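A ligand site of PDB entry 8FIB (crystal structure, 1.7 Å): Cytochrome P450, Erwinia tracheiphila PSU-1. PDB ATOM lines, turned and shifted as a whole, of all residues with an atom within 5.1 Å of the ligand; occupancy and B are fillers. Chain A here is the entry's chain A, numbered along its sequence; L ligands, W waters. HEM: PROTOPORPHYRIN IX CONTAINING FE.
SG of Cys 388 binds FE of the ligand (2.4 Å).
NE2 of His 114 is in hydrogen-bond range of O2D of the ligand (2.7 Å).
A ring nitrogen (ND1) of His 386 lies within hydrogen-bond range of an oxygen (O1D) of the ligand, 2.7 Å away.
NH2 of Arg 320 lies within salt-bridge range of O1A of the ligand (2.8 Å).
The guanidinium group (NH1) of Arg 118 lies within salt-bridge range of an oxygen (O2D) of the ligand (2.8 Å).
The side-chain sulfur (SG) of Cys 388 lies close to the backbone NH (N) of Gly 390 (3.2 Å).
The backbone carbonyl oxygen of Phe 381 lies within hydrogen-bond range of the backbone NH of Cys 388 (2.9 Å).
A ring nitrogen (NE2) of His 114 is in hydrogen-bond range of a ring nitrogen (ND1) of His 386.
The backbone carbonyl oxygen (O) of Phe 387 sits at hydrogen-bond distance from the guanidinium group (NH1) of Arg 118, at 2.7 Å.
The side-chain hydroxyl (OG1) of Thr 270 is in hydrogen-bond range of the backbone carbonyl oxygen (O) of Gly 266 (2.8 Å).
OG of Ser 380 is in hydrogen-bond range of O of Leu 307 (2.6 Å).
A nitrogen (NC) of the ligand sits close to the backbone carbonyl oxygen of Gly 266, at 3.2 Å.
Merely in contact with the ligand: Met 274 (3.0 Å), Ala 107 (3.2 Å), Ser 380 (3.3 Å), Thr 270 (3.4 Å), Ile 318 (3.4 Å), Gly 390 (3.4 Å), Leu 343 (3.5 Å), Ile 263 (3.5 Å), Ile 385 (3.5 Å), Leu 106 (3.5 Å), Phe 381 (3.6 Å), Pro 312 (3.6 Å), Gly 382 (3.6 Å), Thr 271 (3.7 Å), Leu 389 (3.7 Å), Ala 394 (3.7 Å), Gly 267 (3.7 Å), Ser 316 (3.8 Å), Phe 125 (3.9 Å) and Phe 173 (3.96 Å).
26 residues have an atom within 4 Å of the ligand: Leu 106, Ala 107, His 114, Arg 118, Phe 125, Phe 173, Ile 263, Gly 266, Gly 267, Thr 270, Thr 271, Met 274, Pro 312, Ser 316, Ile 318, Arg 320, Leu 343, Ser 380, Phe 381, Gly 382, Ile 385, His 386, Cys 388, Leu 389, Gly 390 and Ala 394.
The nearest printed residue that does not touch the ligand is Leu 71 (4.04 Å).
Water W3 lies within hydrogen-bond range of an oxygen (O1A) of the ligand (2.4 Å), the backbone carbonyl oxygen of His 386 (3.4 Å) and the backbone NH of Phe 387 (3.4 Å).
Water W1 lies within hydrogen-bond range of O2A of the ligand (2.5 Å), N of Ser 317 (2.5 Å) and N of Ile 318 (2.8 Å).
Water W2 bridges the side-chain hydroxyl (OG1) of Thr 271 and the backbone carbonyl oxygen (O) of Gly 267.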
ATOM      1  N   LEU A  71      -7.537  29.962  22.650  1.00  0.00           N
ATOM      2  CA  LEU A  71      -6.948  29.059  23.631  1.00  0.00           C
ATOM      3  C   LEU A  71      -5.968  29.789  24.526  1.00  0.00           C
ATOM      4  O   LEU A  71      -5.916  29.543  25.734  1.00  0.00           O
ATOM      5  CB  LEU A  71      -6.239  27.909  22.939  1.00  0.00           C
ATOM      6  CG  LEU A  71      -7.187  26.969  22.211  1.00  0.00           C
ATOM      7  CD1 LEU A  71      -6.396  26.009  21.323  1.00  0.00           C
ATOM      8  CD2 LEU A  71      -8.074  26.217  23.183  1.00  0.00           C
ATOM      9  N   LEU A 106     -10.894  19.650  36.746  1.00  0.00           N
ATOM     10  CA  LEU A 106      -9.953  20.662  36.292  1.00  0.00           C
ATOM     11  C   LEU A 106     -10.415  21.396  35.038  1.00  0.00           C
ATOM     12  O   LEU A 106     -10.279  22.627  34.941  1.00  0.00           O
ATOM     13  CB  LEU A 106      -8.622  19.937  36.067  1.00  0.00           C
ATOM     14  CG  LEU A 106      -7.300  20.661  35.921  1.00  0.00           C
ATOM     15  CD1 LEU A 106      -7.071  21.556  37.102  1.00  0.00           C
ATOM     16  CD2 LEU A 106      -6.173  19.639  35.755  1.00  0.00           C
ATOM     17  N   ALA A 107     -10.954  20.655  34.076  1.00  0.00           N
ATOM     18  CA  ALA A 107     -11.357  21.246  32.803  1.00  0.00           C
ATOM     19  C   ALA A 107     -12.413  22.331  32.968  1.00  0.00           C
ATOM     20  O   ALA A 107     -12.491  23.243  32.132  1.00  0.00           O
ATOM     21  CB  ALA A 107     -11.850  20.118  31.888  1.00  0.00           C
ATOM     22  N   HIS A 114      -7.931  26.765  39.375  1.00  0.00           N
ATOM     23  CA  HIS A 114      -7.376  25.864  38.385  1.00  0.00           C
ATOM     24  C   HIS A 114      -5.865  25.764  38.511  1.00  0.00           C
ATOM     25  O   HIS A 114      -5.277  24.688  38.360  1.00  0.00           O
ATOM     26  CB  HIS A 114      -7.743  26.350  36.981  1.00  0.00           C
ATOM     27  CG  HIS A 114      -7.097  25.568  35.881  1.00  0.00           C
ATOM     28  ND1 HIS A 114      -5.872  25.901  35.338  1.00  0.00           N
ATOM     29  CD2 HIS A 114      -7.505  24.455  35.225  1.00  0.00           C
ATOM     30  CE1 HIS A 114      -5.547  25.017  34.411  1.00  0.00           C
ATOM     31  NE2 HIS A 114      -6.519  24.134  34.323  1.00  0.00           N
ATOM     32  N   ARG A 118      -3.925  22.294  39.114  1.00  0.00           N
ATOM     33  CA  ARG A 118      -3.024  21.801  38.082  1.00  0.00           C
ATOM     34  C   ARG A 118      -1.608  21.623  38.623  1.00  0.00           C
ATOM     35  O   ARG A 118      -0.940  20.623  38.331  1.00  0.00           O
ATOM     36  CB  ARG A 118      -3.048  22.759  36.892  1.00  0.00           C
ATOM     37  CG  ARG A 118      -2.146  22.324  35.767  1.00  0.00           C
ATOM     38  CD  ARG A 118      -2.893  22.017  34.534  1.00  0.00           C
ATOM     39  NE  ARG A 118      -1.976  21.514  33.517  1.00  0.00           N
ATOM     40  CZ  ARG A 118      -2.358  21.134  32.313  1.00  0.00           C
ATOM     41  NH1 ARG A 118      -3.637  21.182  31.992  1.00  0.00           N
ATOM     42  NH2 ARG A 118      -1.475  20.695  31.440  1.00  0.00           N
ATOM     43  N   PHE A 125       2.033  13.614  38.801  1.00  0.00           N
ATOM     44  CA  PHE A 125       1.766  13.007  37.490  1.00  0.00           C
ATOM     45  C   PHE A 125       2.819  13.591  36.556  1.00  0.00           C
ATOM     46  O   PHE A 125       2.598  14.592  35.879  1.00  0.00           O
ATOM     47  CB  PHE A 125       0.339  13.335  37.062  1.00  0.00           C
ATOM     48  CG  PHE A 125      -0.095  12.685  35.769  1.00  0.00           C
ATOM     49  CD1 PHE A 125       0.172  11.370  35.509  1.00  0.00           C
ATOM     50  CD2 PHE A 125      -0.810  13.414  34.843  1.00  0.00           C
ATOM     51  CE1 PHE A 125      -0.237  10.796  34.320  1.00  0.00           C
ATOM     52  CE2 PHE A 125      -1.225  12.830  33.661  1.00  0.00           C
ATOM     53  CZ  PHE A 125      -0.946  11.527  33.415  1.00  0.00           C
ATOM     54  N   PHE A 173      -4.704   2.991  32.681  1.00  0.00           N
ATOM     55  CA  PHE A 173      -5.215   3.722  33.835  1.00  0.00           C
ATOM     56  C   PHE A 173      -5.226   2.852  35.084  1.00  0.00           C
ATOM     57  O   PHE A 173      -4.909   3.330  36.181  1.00  0.00           O
ATOM     58  CB  PHE A 173      -6.634   4.220  33.563  1.00  0.00           C
ATOM     59  CG  PHE A 173      -6.712   5.547  32.856  1.00  0.00           C
ATOM     60  CD1 PHE A 173      -5.853   6.583  33.178  1.00  0.00           C
ATOM     61  CD2 PHE A 173      -7.684   5.753  31.895  1.00  0.00           C
ATOM     62  CE1 PHE A 173      -5.935   7.796  32.552  1.00  0.00           C
ATOM     63  CE2 PHE A 173      -7.782   6.981  31.263  1.00  0.00           C
ATOM     64  CZ  PHE A 173      -6.898   8.004  31.588  1.00  0.00           C
ATOM     65  N   GLY A 262     -11.630  13.277  36.772  1.00  0.00           N
ATOM     66  CA  GLY A 262     -11.383  14.077  35.584  1.00  0.00           C
ATOM     67  C   GLY A 262     -10.322  13.508  34.676  1.00  0.00           C
ATOM     68  O   GLY A 262     -10.427  13.626  33.448  1.00  0.00           O
ATOM     69  N   ILE A 263      -9.301  12.870  35.263  1.00  0.00           N
ATOM     70  CA  ILE A 263      -8.281  12.174  34.484  1.00  0.00           C
ATOM     71  C   ILE A 263      -8.905  11.036  33.691  1.00  0.00           C
ATOM     72  O   ILE A 263      -8.635  10.865  32.502  1.00  0.00           O
ATOM     73  CB  ILE A 263      -7.151  11.682  35.401  1.00  0.00           C
ATOM     74  CG1 ILE A 263      -6.277  12.861  35.847  1.00  0.00           C
ATOM     75  CG2 ILE A 263      -6.327  10.613  34.690  1.00  0.00           C
ATOM     76  CD1 ILE A 263      -5.342  12.591  37.028  1.00  0.00           C
ATOM     77  N   GLY A 266     -10.999  12.404  30.908  1.00  0.00           N
ATOM     78  CA  GLY A 266     -10.166  12.963  29.860  1.00  0.00           C
ATOM     79  C   GLY A 266      -9.637  11.919  28.889  1.00  0.00           C
ATOM     80  O   GLY A 266      -9.499  12.180  27.688  1.00  0.00           O
ATOM     81  N   GLY A 267      -9.295  10.736  29.408  1.00  0.00           N
ATOM     82  CA  GLY A 267      -8.793   9.643  28.635  1.00  0.00           C
ATOM     83  C   GLY A 267      -9.815   8.592  28.290  1.00  0.00           C
ATOM     84  O   GLY A 267      -9.448   7.542  27.738  1.00  0.00           O
ATOM     85  N   THR A 270     -10.939   9.247  24.149  1.00  0.00           N
ATOM     86  CA  THR A 270     -10.015   9.991  23.293  1.00  0.00           C
ATOM     87  C   THR A 270      -8.851   9.128  22.837  1.00  0.00           C
ATOM     88  O   THR A 270      -8.567   9.028  21.639  1.00  0.00           O
ATOM     89  CB  THR A 270      -9.513  11.202  24.087  1.00  0.00           C
ATOM     90  OG1 THR A 270      -9.052  10.743  25.365  1.00  0.00           O
ATOM     91  CG2 THR A 270     -10.643  12.188  24.323  1.00  0.00           C
ATOM     92  N   THR A 271      -8.151   8.502  23.788  1.00  0.00           N
ATOM     93  CA  THR A 271      -7.008   7.667  23.424  1.00  0.00           C
ATOM     94  C   THR A 271      -7.417   6.516  22.520  1.00  0.00           C
ATOM     95  O   THR A 271      -6.723   6.216  21.549  1.00  0.00           O
ATOM     96  CB  THR A 271      -6.347   7.157  24.688  1.00  0.00           C
ATOM     97  OG1 THR A 271      -6.090   8.291  25.534  1.00  0.00           O
ATOM     98  CG2 THR A 271      -5.059   6.476  24.350  1.00  0.00           C
ATOM     99  N   MET A 274      -7.803   7.861  19.079  1.00  0.00           N
ATOM    100  CA  MET A 274      -6.447   8.100  18.582  1.00  0.00           C
ATOM    101  C   MET A 274      -5.838   6.806  18.052  1.00  0.00           C
ATOM    102  O   MET A 274      -5.320   6.765  16.932  1.00  0.00           O
ATOM    103  CB  MET A 274      -5.614   8.682  19.731  1.00  0.00           C
ATOM    104  CG  MET A 274      -4.208   9.206  19.397  1.00  0.00           C
ATOM    105  SD  MET A 274      -3.283   9.782  20.851  1.00  0.00           S
ATOM    106  CE  MET A 274      -1.602   9.755  20.317  1.00  0.00           C
ATOM    107  N   LEU A 307      -2.271  12.693  15.069  1.00  0.00           N
ATOM    108  CA  LEU A 307      -3.013  13.677  15.853  1.00  0.00           C
ATOM    109  C   LEU A 307      -3.421  14.885  15.025  1.00  0.00           C
ATOM    110  O   LEU A 307      -4.521  15.423  15.205  1.00  0.00           O
ATOM    111  CB  LEU A 307      -2.140  14.108  17.026  1.00  0.00           C
ATOM    112  CG  LEU A 307      -1.966  13.076  18.129  1.00  0.00           C
ATOM    113  CD1 LEU A 307      -0.728  13.418  18.919  1.00  0.00           C
ATOM    114  CD2 LEU A 307      -3.191  13.039  19.002  1.00  0.00           C
ATOM    115  N   PRO A 312     -10.620  13.418  18.378  1.00  0.00           N
ATOM    116  CA  PRO A 312     -11.716  12.616  18.932  1.00  0.00           C
ATOM    117  C   PRO A 312     -12.994  13.386  19.227  1.00  0.00           C
ATOM    118  O   PRO A 312     -14.065  12.768  19.326  1.00  0.00           O
ATOM    119  CB  PRO A 312     -11.127  12.035  20.227  1.00  0.00           C
ATOM    120  CG  PRO A 312      -9.740  12.637  20.390  1.00  0.00           C
ATOM    121  CD  PRO A 312      -9.590  13.735  19.382  1.00  0.00           C
ATOM    122  N   SER A 316     -14.751  21.735  20.790  1.00  0.00           N
ATOM    123  CA  SER A 316     -14.258  21.698  22.164  1.00  0.00           C
ATOM    124  C   SER A 316     -15.381  21.517  23.165  1.00  0.00           C
ATOM    125  O   SER A 316     -16.513  21.967  22.956  1.00  0.00           O
ATOM    126  CB  SER A 316     -13.490  22.998  22.486  1.00  0.00           C
ATOM    127  OG  SER A 316     -14.273  24.155  22.256  1.00  0.00           O
ATOM    128  N   SER A 317     -15.040  20.853  24.279  1.00  0.00           N
ATOM    129  CA  SER A 317     -16.000  20.600  25.342  1.00  0.00           C
ATOM    130  C   SER A 317     -15.941  21.648  26.460  1.00  0.00           C
ATOM    131  O   SER A 317     -16.924  21.846  27.176  1.00  0.00           O
ATOM    132  CB  SER A 317     -15.719  19.221  25.940  1.00  0.00           C
ATOM    133  OG  SER A 317     -16.669  18.923  26.934  1.00  0.00           O
ATOM    134  N   ILE A 318     -14.810  22.316  26.638  1.00  0.00           N
ATOM    135  CA  ILE A 318     -14.700  23.283  27.725  1.00  0.00           C
ATOM    136  C   ILE A 318     -15.377  24.590  27.319  1.00  0.00           C
ATOM    137  O   ILE A 318     -14.998  25.175  26.307  1.00  0.00           O
ATOM    138  CB  ILE A 318     -13.227  23.537  28.093  1.00  0.00           C
ATOM    139  CG1 ILE A 318     -12.548  22.236  28.509  1.00  0.00           C
ATOM    140  CG2 ILE A 318     -13.104  24.594  29.183  1.00  0.00           C
ATOM    141  CD1 ILE A 318     -11.085  22.415  28.899  1.00  0.00           C
ATOM    142  N   ARG A 320     -15.866  28.446  27.078  1.00  0.00           N
ATOM    143  CA  ARG A 320     -15.041  29.645  27.192  1.00  0.00           C
ATOM    144  C   ARG A 320     -15.998  30.820  27.074  1.00  0.00           C
ATOM    145  O   ARG A 320     -16.599  31.040  26.009  1.00  0.00           O
ATOM    146  CB  ARG A 320     -13.947  29.672  26.123  1.00  0.00           C
ATOM    147  CG  ARG A 320     -12.838  28.681  26.388  1.00  0.00           C
ATOM    148  CD  ARG A 320     -11.787  28.591  25.267  1.00  0.00           C
ATOM    149  NE  ARG A 320     -10.636  27.886  25.813  1.00  0.00           N
ATOM    150  CZ  ARG A 320     -10.490  26.567  25.857  1.00  0.00           C
ATOM    151  NH1 ARG A 320     -11.434  25.783  25.329  1.00  0.00           N
ATOM    152  NH2 ARG A 320      -9.419  26.027  26.436  1.00  0.00           N
ATOM    153  N   LEU A 343     -10.850  22.202  16.724  1.00  0.00           N
ATOM    154  CA  LEU A 343      -9.423  21.878  16.691  1.00  0.00           C
ATOM    155  C   LEU A 343      -9.033  21.145  15.417  1.00  0.00           C
ATOM    156  O   LEU A 343      -7.948  21.386  14.869  1.00  0.00           O
ATOM    157  CB  LEU A 343      -9.065  21.037  17.908  1.00  0.00           C
ATOM    158  CG  LEU A 343      -9.399  21.611  19.292  1.00  0.00           C
ATOM    159  CD1 LEU A 343      -9.201  20.524  20.364  1.00  0.00           C
ATOM    160  CD2 LEU A 343      -8.516  22.788  19.549  1.00  0.00           C
ATOM    161  N   LEU A 379      -2.915  21.490  17.262  1.00  0.00           N
ATOM    162  CA  LEU A 379      -3.961  21.922  18.190  1.00  0.00           C
ATOM    163  C   LEU A 379      -4.723  20.765  18.853  1.00  0.00           C
ATOM    164  O   LEU A 379      -5.635  21.027  19.636  1.00  0.00           O
ATOM    165  CB  LEU A 379      -4.982  22.828  17.479  1.00  0.00           C
ATOM    166  CG  LEU A 379      -4.407  24.103  16.883  1.00  0.00           C
ATOM    167  CD1 LEU A 379      -5.470  24.801  16.056  1.00  0.00           C
ATOM    168  CD2 LEU A 379      -3.845  25.058  17.938  1.00  0.00           C
ATOM    169  N   SER A 380      -4.319  19.518  18.600  1.00  0.00           N
ATOM    170  CA  SER A 380      -5.095  18.373  19.046  1.00  0.00           C
ATOM    171  C   SER A 380      -5.219  18.272  20.561  1.00  0.00           C
ATOM    172  O   SER A 380      -6.173  17.656  21.052  1.00  0.00           O
ATOM    173  CB  SER A 380      -4.451  17.110  18.480  1.00  0.00           C
ATOM    174  OG  SER A 380      -4.358  17.192  17.064  1.00  0.00           O
ATOM    175  N   PHE A 381      -4.280  18.847  21.309  1.00  0.00           N
ATOM    176  CA  PHE A 381      -4.324  18.841  22.766  1.00  0.00           C
ATOM    177  C   PHE A 381      -4.672  20.195  23.358  1.00  0.00           C
ATOM    178  O   PHE A 381      -4.547  20.397  24.569  1.00  0.00           O
ATOM    179  CB  PHE A 381      -2.971  18.379  23.310  1.00  0.00           C
ATOM    180  CG  PHE A 381      -2.667  16.930  23.041  1.00  0.00           C
ATOM    181  CD1 PHE A 381      -3.494  15.911  23.515  1.00  0.00           C
ATOM    182  CD2 PHE A 381      -1.505  16.589  22.356  1.00  0.00           C
ATOM    183  CE1 PHE A 381      -3.166  14.569  23.295  1.00  0.00           C
ATOM    184  CE2 PHE A 381      -1.188  15.258  22.144  1.00  0.00           C
ATOM    185  CZ  PHE A 381      -2.014  14.253  22.598  1.00  0.00           C
ATOM    186  N   GLY A 382      -5.123  21.128  22.536  1.00  0.00           N
ATOM    187  CA  GLY A 382      -5.376  22.465  23.005  1.00  0.00           C
ATOM    188  C   GLY A 382      -4.095  23.258  23.131  1.00  0.00           C
ATOM    189  O   GLY A 382      -3.068  22.952  22.519  1.00  0.00           O
ATOM    190  N   ILE A 385      -3.745  27.344  29.234  1.00  0.00           N
ATOM    191  CA  ILE A 385      -3.815  26.803  30.602  1.00  0.00           C
ATOM    192  C   ILE A 385      -4.556  25.466  30.663  1.00  0.00           C
ATOM    193  O   ILE A 385      -4.328  24.692  31.604  1.00  0.00           O
ATOM    194  CB  ILE A 385      -4.429  27.797  31.606  1.00  0.00           C
ATOM    195  CG1 ILE A 385      -5.902  28.094  31.286  1.00  0.00           C
ATOM    196  CG2 ILE A 385      -3.592  29.052  31.659  1.00  0.00           C
ATOM    197  CD1 ILE A 385      -6.598  28.893  32.407  1.00  0.00           C
ATOM    198  N   HIS A 386      -5.451  25.168  29.732  1.00  0.00           N
ATOM    199  CA  HIS A 386      -6.157  23.880  29.770  1.00  0.00           C
ATOM    200  C   HIS A 386      -5.538  22.839  28.853  1.00  0.00           C
ATOM    201  O   HIS A 386      -6.165  21.815  28.567  1.00  0.00           O
ATOM    202  CB  HIS A 386      -7.652  24.067  29.437  1.00  0.00           C
ATOM    203  CG  HIS A 386      -8.391  24.908  30.446  1.00  0.00           C
ATOM    204  ND1 HIS A 386      -8.695  24.459  31.705  1.00  0.00           N
ATOM    205  CD2 HIS A 386      -8.867  26.179  30.368  1.00  0.00           C
ATOM    206  CE1 HIS A 386      -9.311  25.409  32.382  1.00  0.00           C
ATOM    207  NE2 HIS A 386      -9.440  26.471  31.595  1.00  0.00           N
ATOM    208  N   PHE A 387      -4.312  23.062  28.374  1.00  0.00           N
ATOM    209  CA  PHE A 387      -3.628  22.079  27.541  1.00  0.00           C
ATOM    210  C   PHE A 387      -3.721  20.688  28.161  1.00  0.00           C
ATOM    211  O   PHE A 387      -3.508  20.525  29.364  1.00  0.00           O
ATOM    212  CB  PHE A 387      -2.180  22.518  27.356  1.00  0.00           C
ATOM    213  CG  PHE A 387      -1.373  21.577  26.536  1.00  0.00           C
ATOM    214  CD1 PHE A 387      -0.661  20.566  27.137  1.00  0.00           C
ATOM    215  CD2 PHE A 387      -1.322  21.696  25.152  1.00  0.00           C
ATOM    216  CE1 PHE A 387       0.085  19.694  26.380  1.00  0.00           C
ATOM    217  CE2 PHE A 387      -0.588  20.830  24.393  1.00  0.00           C
ATOM    218  CZ  PHE A 387       0.122  19.833  24.998  1.00  0.00           C
ATOM    219  N   CYS A 388      -4.054  19.699  27.348  1.00  0.00           N
ATOM    220  CA  CYS A 388      -4.353  18.360  27.854  1.00  0.00           C
ATOM    221  C   CYS A 388      -3.368  17.888  28.912  1.00  0.00           C
ATOM    222  O   CYS A 388      -2.166  17.785  28.644  1.00  0.00           O
ATOM    223  CB  CYS A 388      -4.358  17.374  26.678  1.00  0.00           C
ATOM    224  SG  CYS A 388      -4.640  15.700  27.170  1.00  0.00           S
ATOM    225  N   LEU A 389      -3.885  17.563  30.085  1.00  0.00           N
ATOM    226  CA  LEU A 389      -3.040  17.018  31.151  1.00  0.00           C
ATOM    227  C   LEU A 389      -2.428  15.686  30.749  1.00  0.00           C
ATOM    228  O   LEU A 389      -1.336  15.333  31.213  1.00  0.00           O
ATOM    229  CB  LEU A 389      -3.871  16.839  32.419  1.00  0.00           C
ATOM    230  CG  LEU A 389      -3.082  16.473  33.682  1.00  0.00           C
ATOM    231  CD1 LEU A 389      -2.299  17.695  34.140  1.00  0.00           C
ATOM    232  CD2 LEU A 389      -3.990  15.966  34.769  1.00  0.00           C
ATOM    233  N   GLY A 390      -3.131  14.938  29.912  1.00  0.00           N
ATOM    234  CA  GLY A 390      -2.679  13.620  29.517  1.00  0.00           C
ATOM    235  C   GLY A 390      -1.923  13.543  28.203  1.00  0.00           C
ATOM    236  O   GLY A 390      -1.778  12.451  27.665  1.00  0.00           O
ATOM    237  N   LEU A 393       0.895  11.096  28.215  1.00  0.00           N
ATOM    238  CA  LEU A 393       0.388   9.737  28.403  1.00  0.00           C
ATOM    239  C   LEU A 393      -0.217   9.190  27.113  1.00  0.00           C
ATOM    240  O   LEU A 393       0.007   8.033  26.754  1.00  0.00           O
ATOM    241  CB  LEU A 393      -0.622   9.726  29.554  1.00  0.00           C
ATOM    242  CG  LEU A 393      -1.292   8.387  29.851  1.00  0.00           C
ATOM    243  CD1 LEU A 393      -0.273   7.303  30.139  1.00  0.00           C
ATOM    244  CD2 LEU A 393      -2.269   8.513  31.033  1.00  0.00           C
ATOM    245  N   ALA A 394      -0.994  10.015  26.410  1.00  0.00           N
ATOM    246  CA  ALA A 394      -1.536   9.579  25.126  1.00  0.00           C
ATOM    247  C   ALA A 394      -0.430   9.325  24.105  1.00  0.00           C
ATOM    248  O   ALA A 394      -0.434   8.307  23.407  1.00  0.00           O
ATOM    249  CB  ALA A 394      -2.511  10.628  24.605  1.00  0.00           C
ATOM    250  N   GLN A 397       1.495   6.054  24.981  1.00  0.00           N
ATOM    251  CA  GLN A 397       0.711   4.857  24.684  1.00  0.00           C
ATOM    252  C   GLN A 397       0.764   4.538  23.195  1.00  0.00           C
ATOM    253  O   GLN A 397       0.959   3.378  22.807  1.00  0.00           O
ATOM    254  CB  GLN A 397      -0.745   5.039  25.123  1.00  0.00           C
ATOM    255  CG  GLN A 397      -0.944   4.879  26.627  1.00  0.00           C
ATOM    256  CD  GLN A 397      -2.395   4.925  27.053  1.00  0.00           C
ATOM    257  OE1 GLN A 397      -3.165   3.993  26.819  1.00  0.00           O
ATOM    258  NE2 GLN A 397      -2.769   6.012  27.679  1.00  0.00           N
HETATM  259  CHA HEM L   1      -7.812  18.537  28.301  1.00  0.00           C
HETATM  260  CHB HEM L   1      -7.555  16.201  24.065  1.00  0.00           C
HETATM  261  CHC HEM L   1      -6.137  12.194  26.344  1.00  0.00           C
HETATM  262  CHD HEM L   1      -6.828  14.373  30.617  1.00  0.00           C
HETATM  263  C1A HEM L   1      -7.800  18.272  26.963  1.00  0.00           C
HETATM  264  C2A HEM L   1      -7.995  19.227  25.910  1.00  0.00           C
HETATM  265  C3A HEM L   1      -7.927  18.565  24.753  1.00  0.00           C
HETATM  266  C4A HEM L   1      -7.684  17.166  25.028  1.00  0.00           C
HETATM  267  CMA HEM L   1      -8.071  19.143  23.339  1.00  0.00           C
HETATM  268  CAA HEM L   1      -8.209  20.741  26.102  1.00  0.00           C
HETATM  269  CBA HEM L   1      -9.642  21.084  25.772  1.00  0.00           C
HETATM  270  CGA HEM L   1      -9.843  22.574  25.706  1.00  0.00           C
HETATM  271  O1A HEM L   1      -8.872  23.362  25.933  1.00  0.00           O
HETATM  272  O2A HEM L   1     -11.012  22.935  25.379  1.00  0.00           O
HETATM  273  C1B HEM L   1      -7.114  14.939  24.320  1.00  0.00           C
HETATM  274  C2B HEM L   1      -6.769  13.967  23.324  1.00  0.00           C
HETATM  275  C3B HEM L   1      -6.393  12.872  23.985  1.00  0.00           C
HETATM  276  C4B HEM L   1      -6.465  13.116  25.392  1.00  0.00           C
HETATM  277  CMB HEM L   1      -6.857  14.203  21.811  1.00  0.00           C
HETATM  278  CAB HEM L   1      -5.908  11.536  23.441  1.00  0.00           C
HETATM  279  CBB HEM L   1      -5.271  11.531  22.280  1.00  0.00           C
HETATM  280  C1C HEM L   1      -6.120  12.438  27.689  1.00  0.00           C
HETATM  281  C2C HEM L   1      -5.609  11.550  28.709  1.00  0.00           C
HETATM  282  C3C HEM L   1      -5.783  12.179  29.880  1.00  0.00           C
HETATM  283  C4C HEM L   1      -6.440  13.448  29.657  1.00  0.00           C
HETATM  284  CMC HEM L   1      -4.932  10.190  28.431  1.00  0.00           C
HETATM  285  CAC HEM L   1      -5.359  11.641  31.259  1.00  0.00           C
HETATM  286  CBC HEM L   1      -4.817  12.482  32.161  1.00  0.00           C
HETATM  287  C1D HEM L   1      -7.177  15.688  30.351  1.00  0.00           C
HETATM  288  C2D HEM L   1      -7.499  16.688  31.337  1.00  0.00           C
HETATM  289  C3D HEM L   1      -7.765  17.841  30.730  1.00  0.00           C
HETATM  290  C4D HEM L   1      -7.630  17.601  29.286  1.00  0.00           C
HETATM  291  CMD HEM L   1      -7.500  16.417  32.850  1.00  0.00           C
HETATM  292  CAD HEM L   1      -8.129  19.175  31.431  1.00  0.00           C
HETATM  293  CBD HEM L   1      -6.852  20.004  31.606  1.00  0.00           C
HETATM  294  CGD HEM L   1      -7.140  21.354  32.214  1.00  0.00           C
HETATM  295  O1D HEM L   1      -8.296  21.846  32.101  1.00  0.00           O
HETATM  296  O2D HEM L   1      -6.226  21.967  32.802  1.00  0.00           O
HETATM  297  NA  HEM L   1      -7.602  17.009  26.401  1.00  0.00           N
HETATM  298  NB  HEM L   1      -6.909  14.408  25.578  1.00  0.00           N
HETATM  299  NC  HEM L   1      -6.628  13.573  28.297  1.00  0.00           N
HETATM  300  ND  HEM L   1      -7.275  16.275  29.100  1.00  0.00           N
HETATM  301 FE   HEM L   1      -6.965  15.350  27.342  1.00  0.00          FE
HETATM  302  O   HOH W   1     -12.700  21.171  25.135  1.00  0.00           O
HETATM  303  O   HOH W   2      -6.552   7.244  27.892  1.00  0.00           O
HETATM  304  O   HOH W   3      -6.489  23.885  25.907  1.00  0.00           O
HETATM  305  O   HOH W   4      -9.264  14.792  27.375  1.00  0.00           O
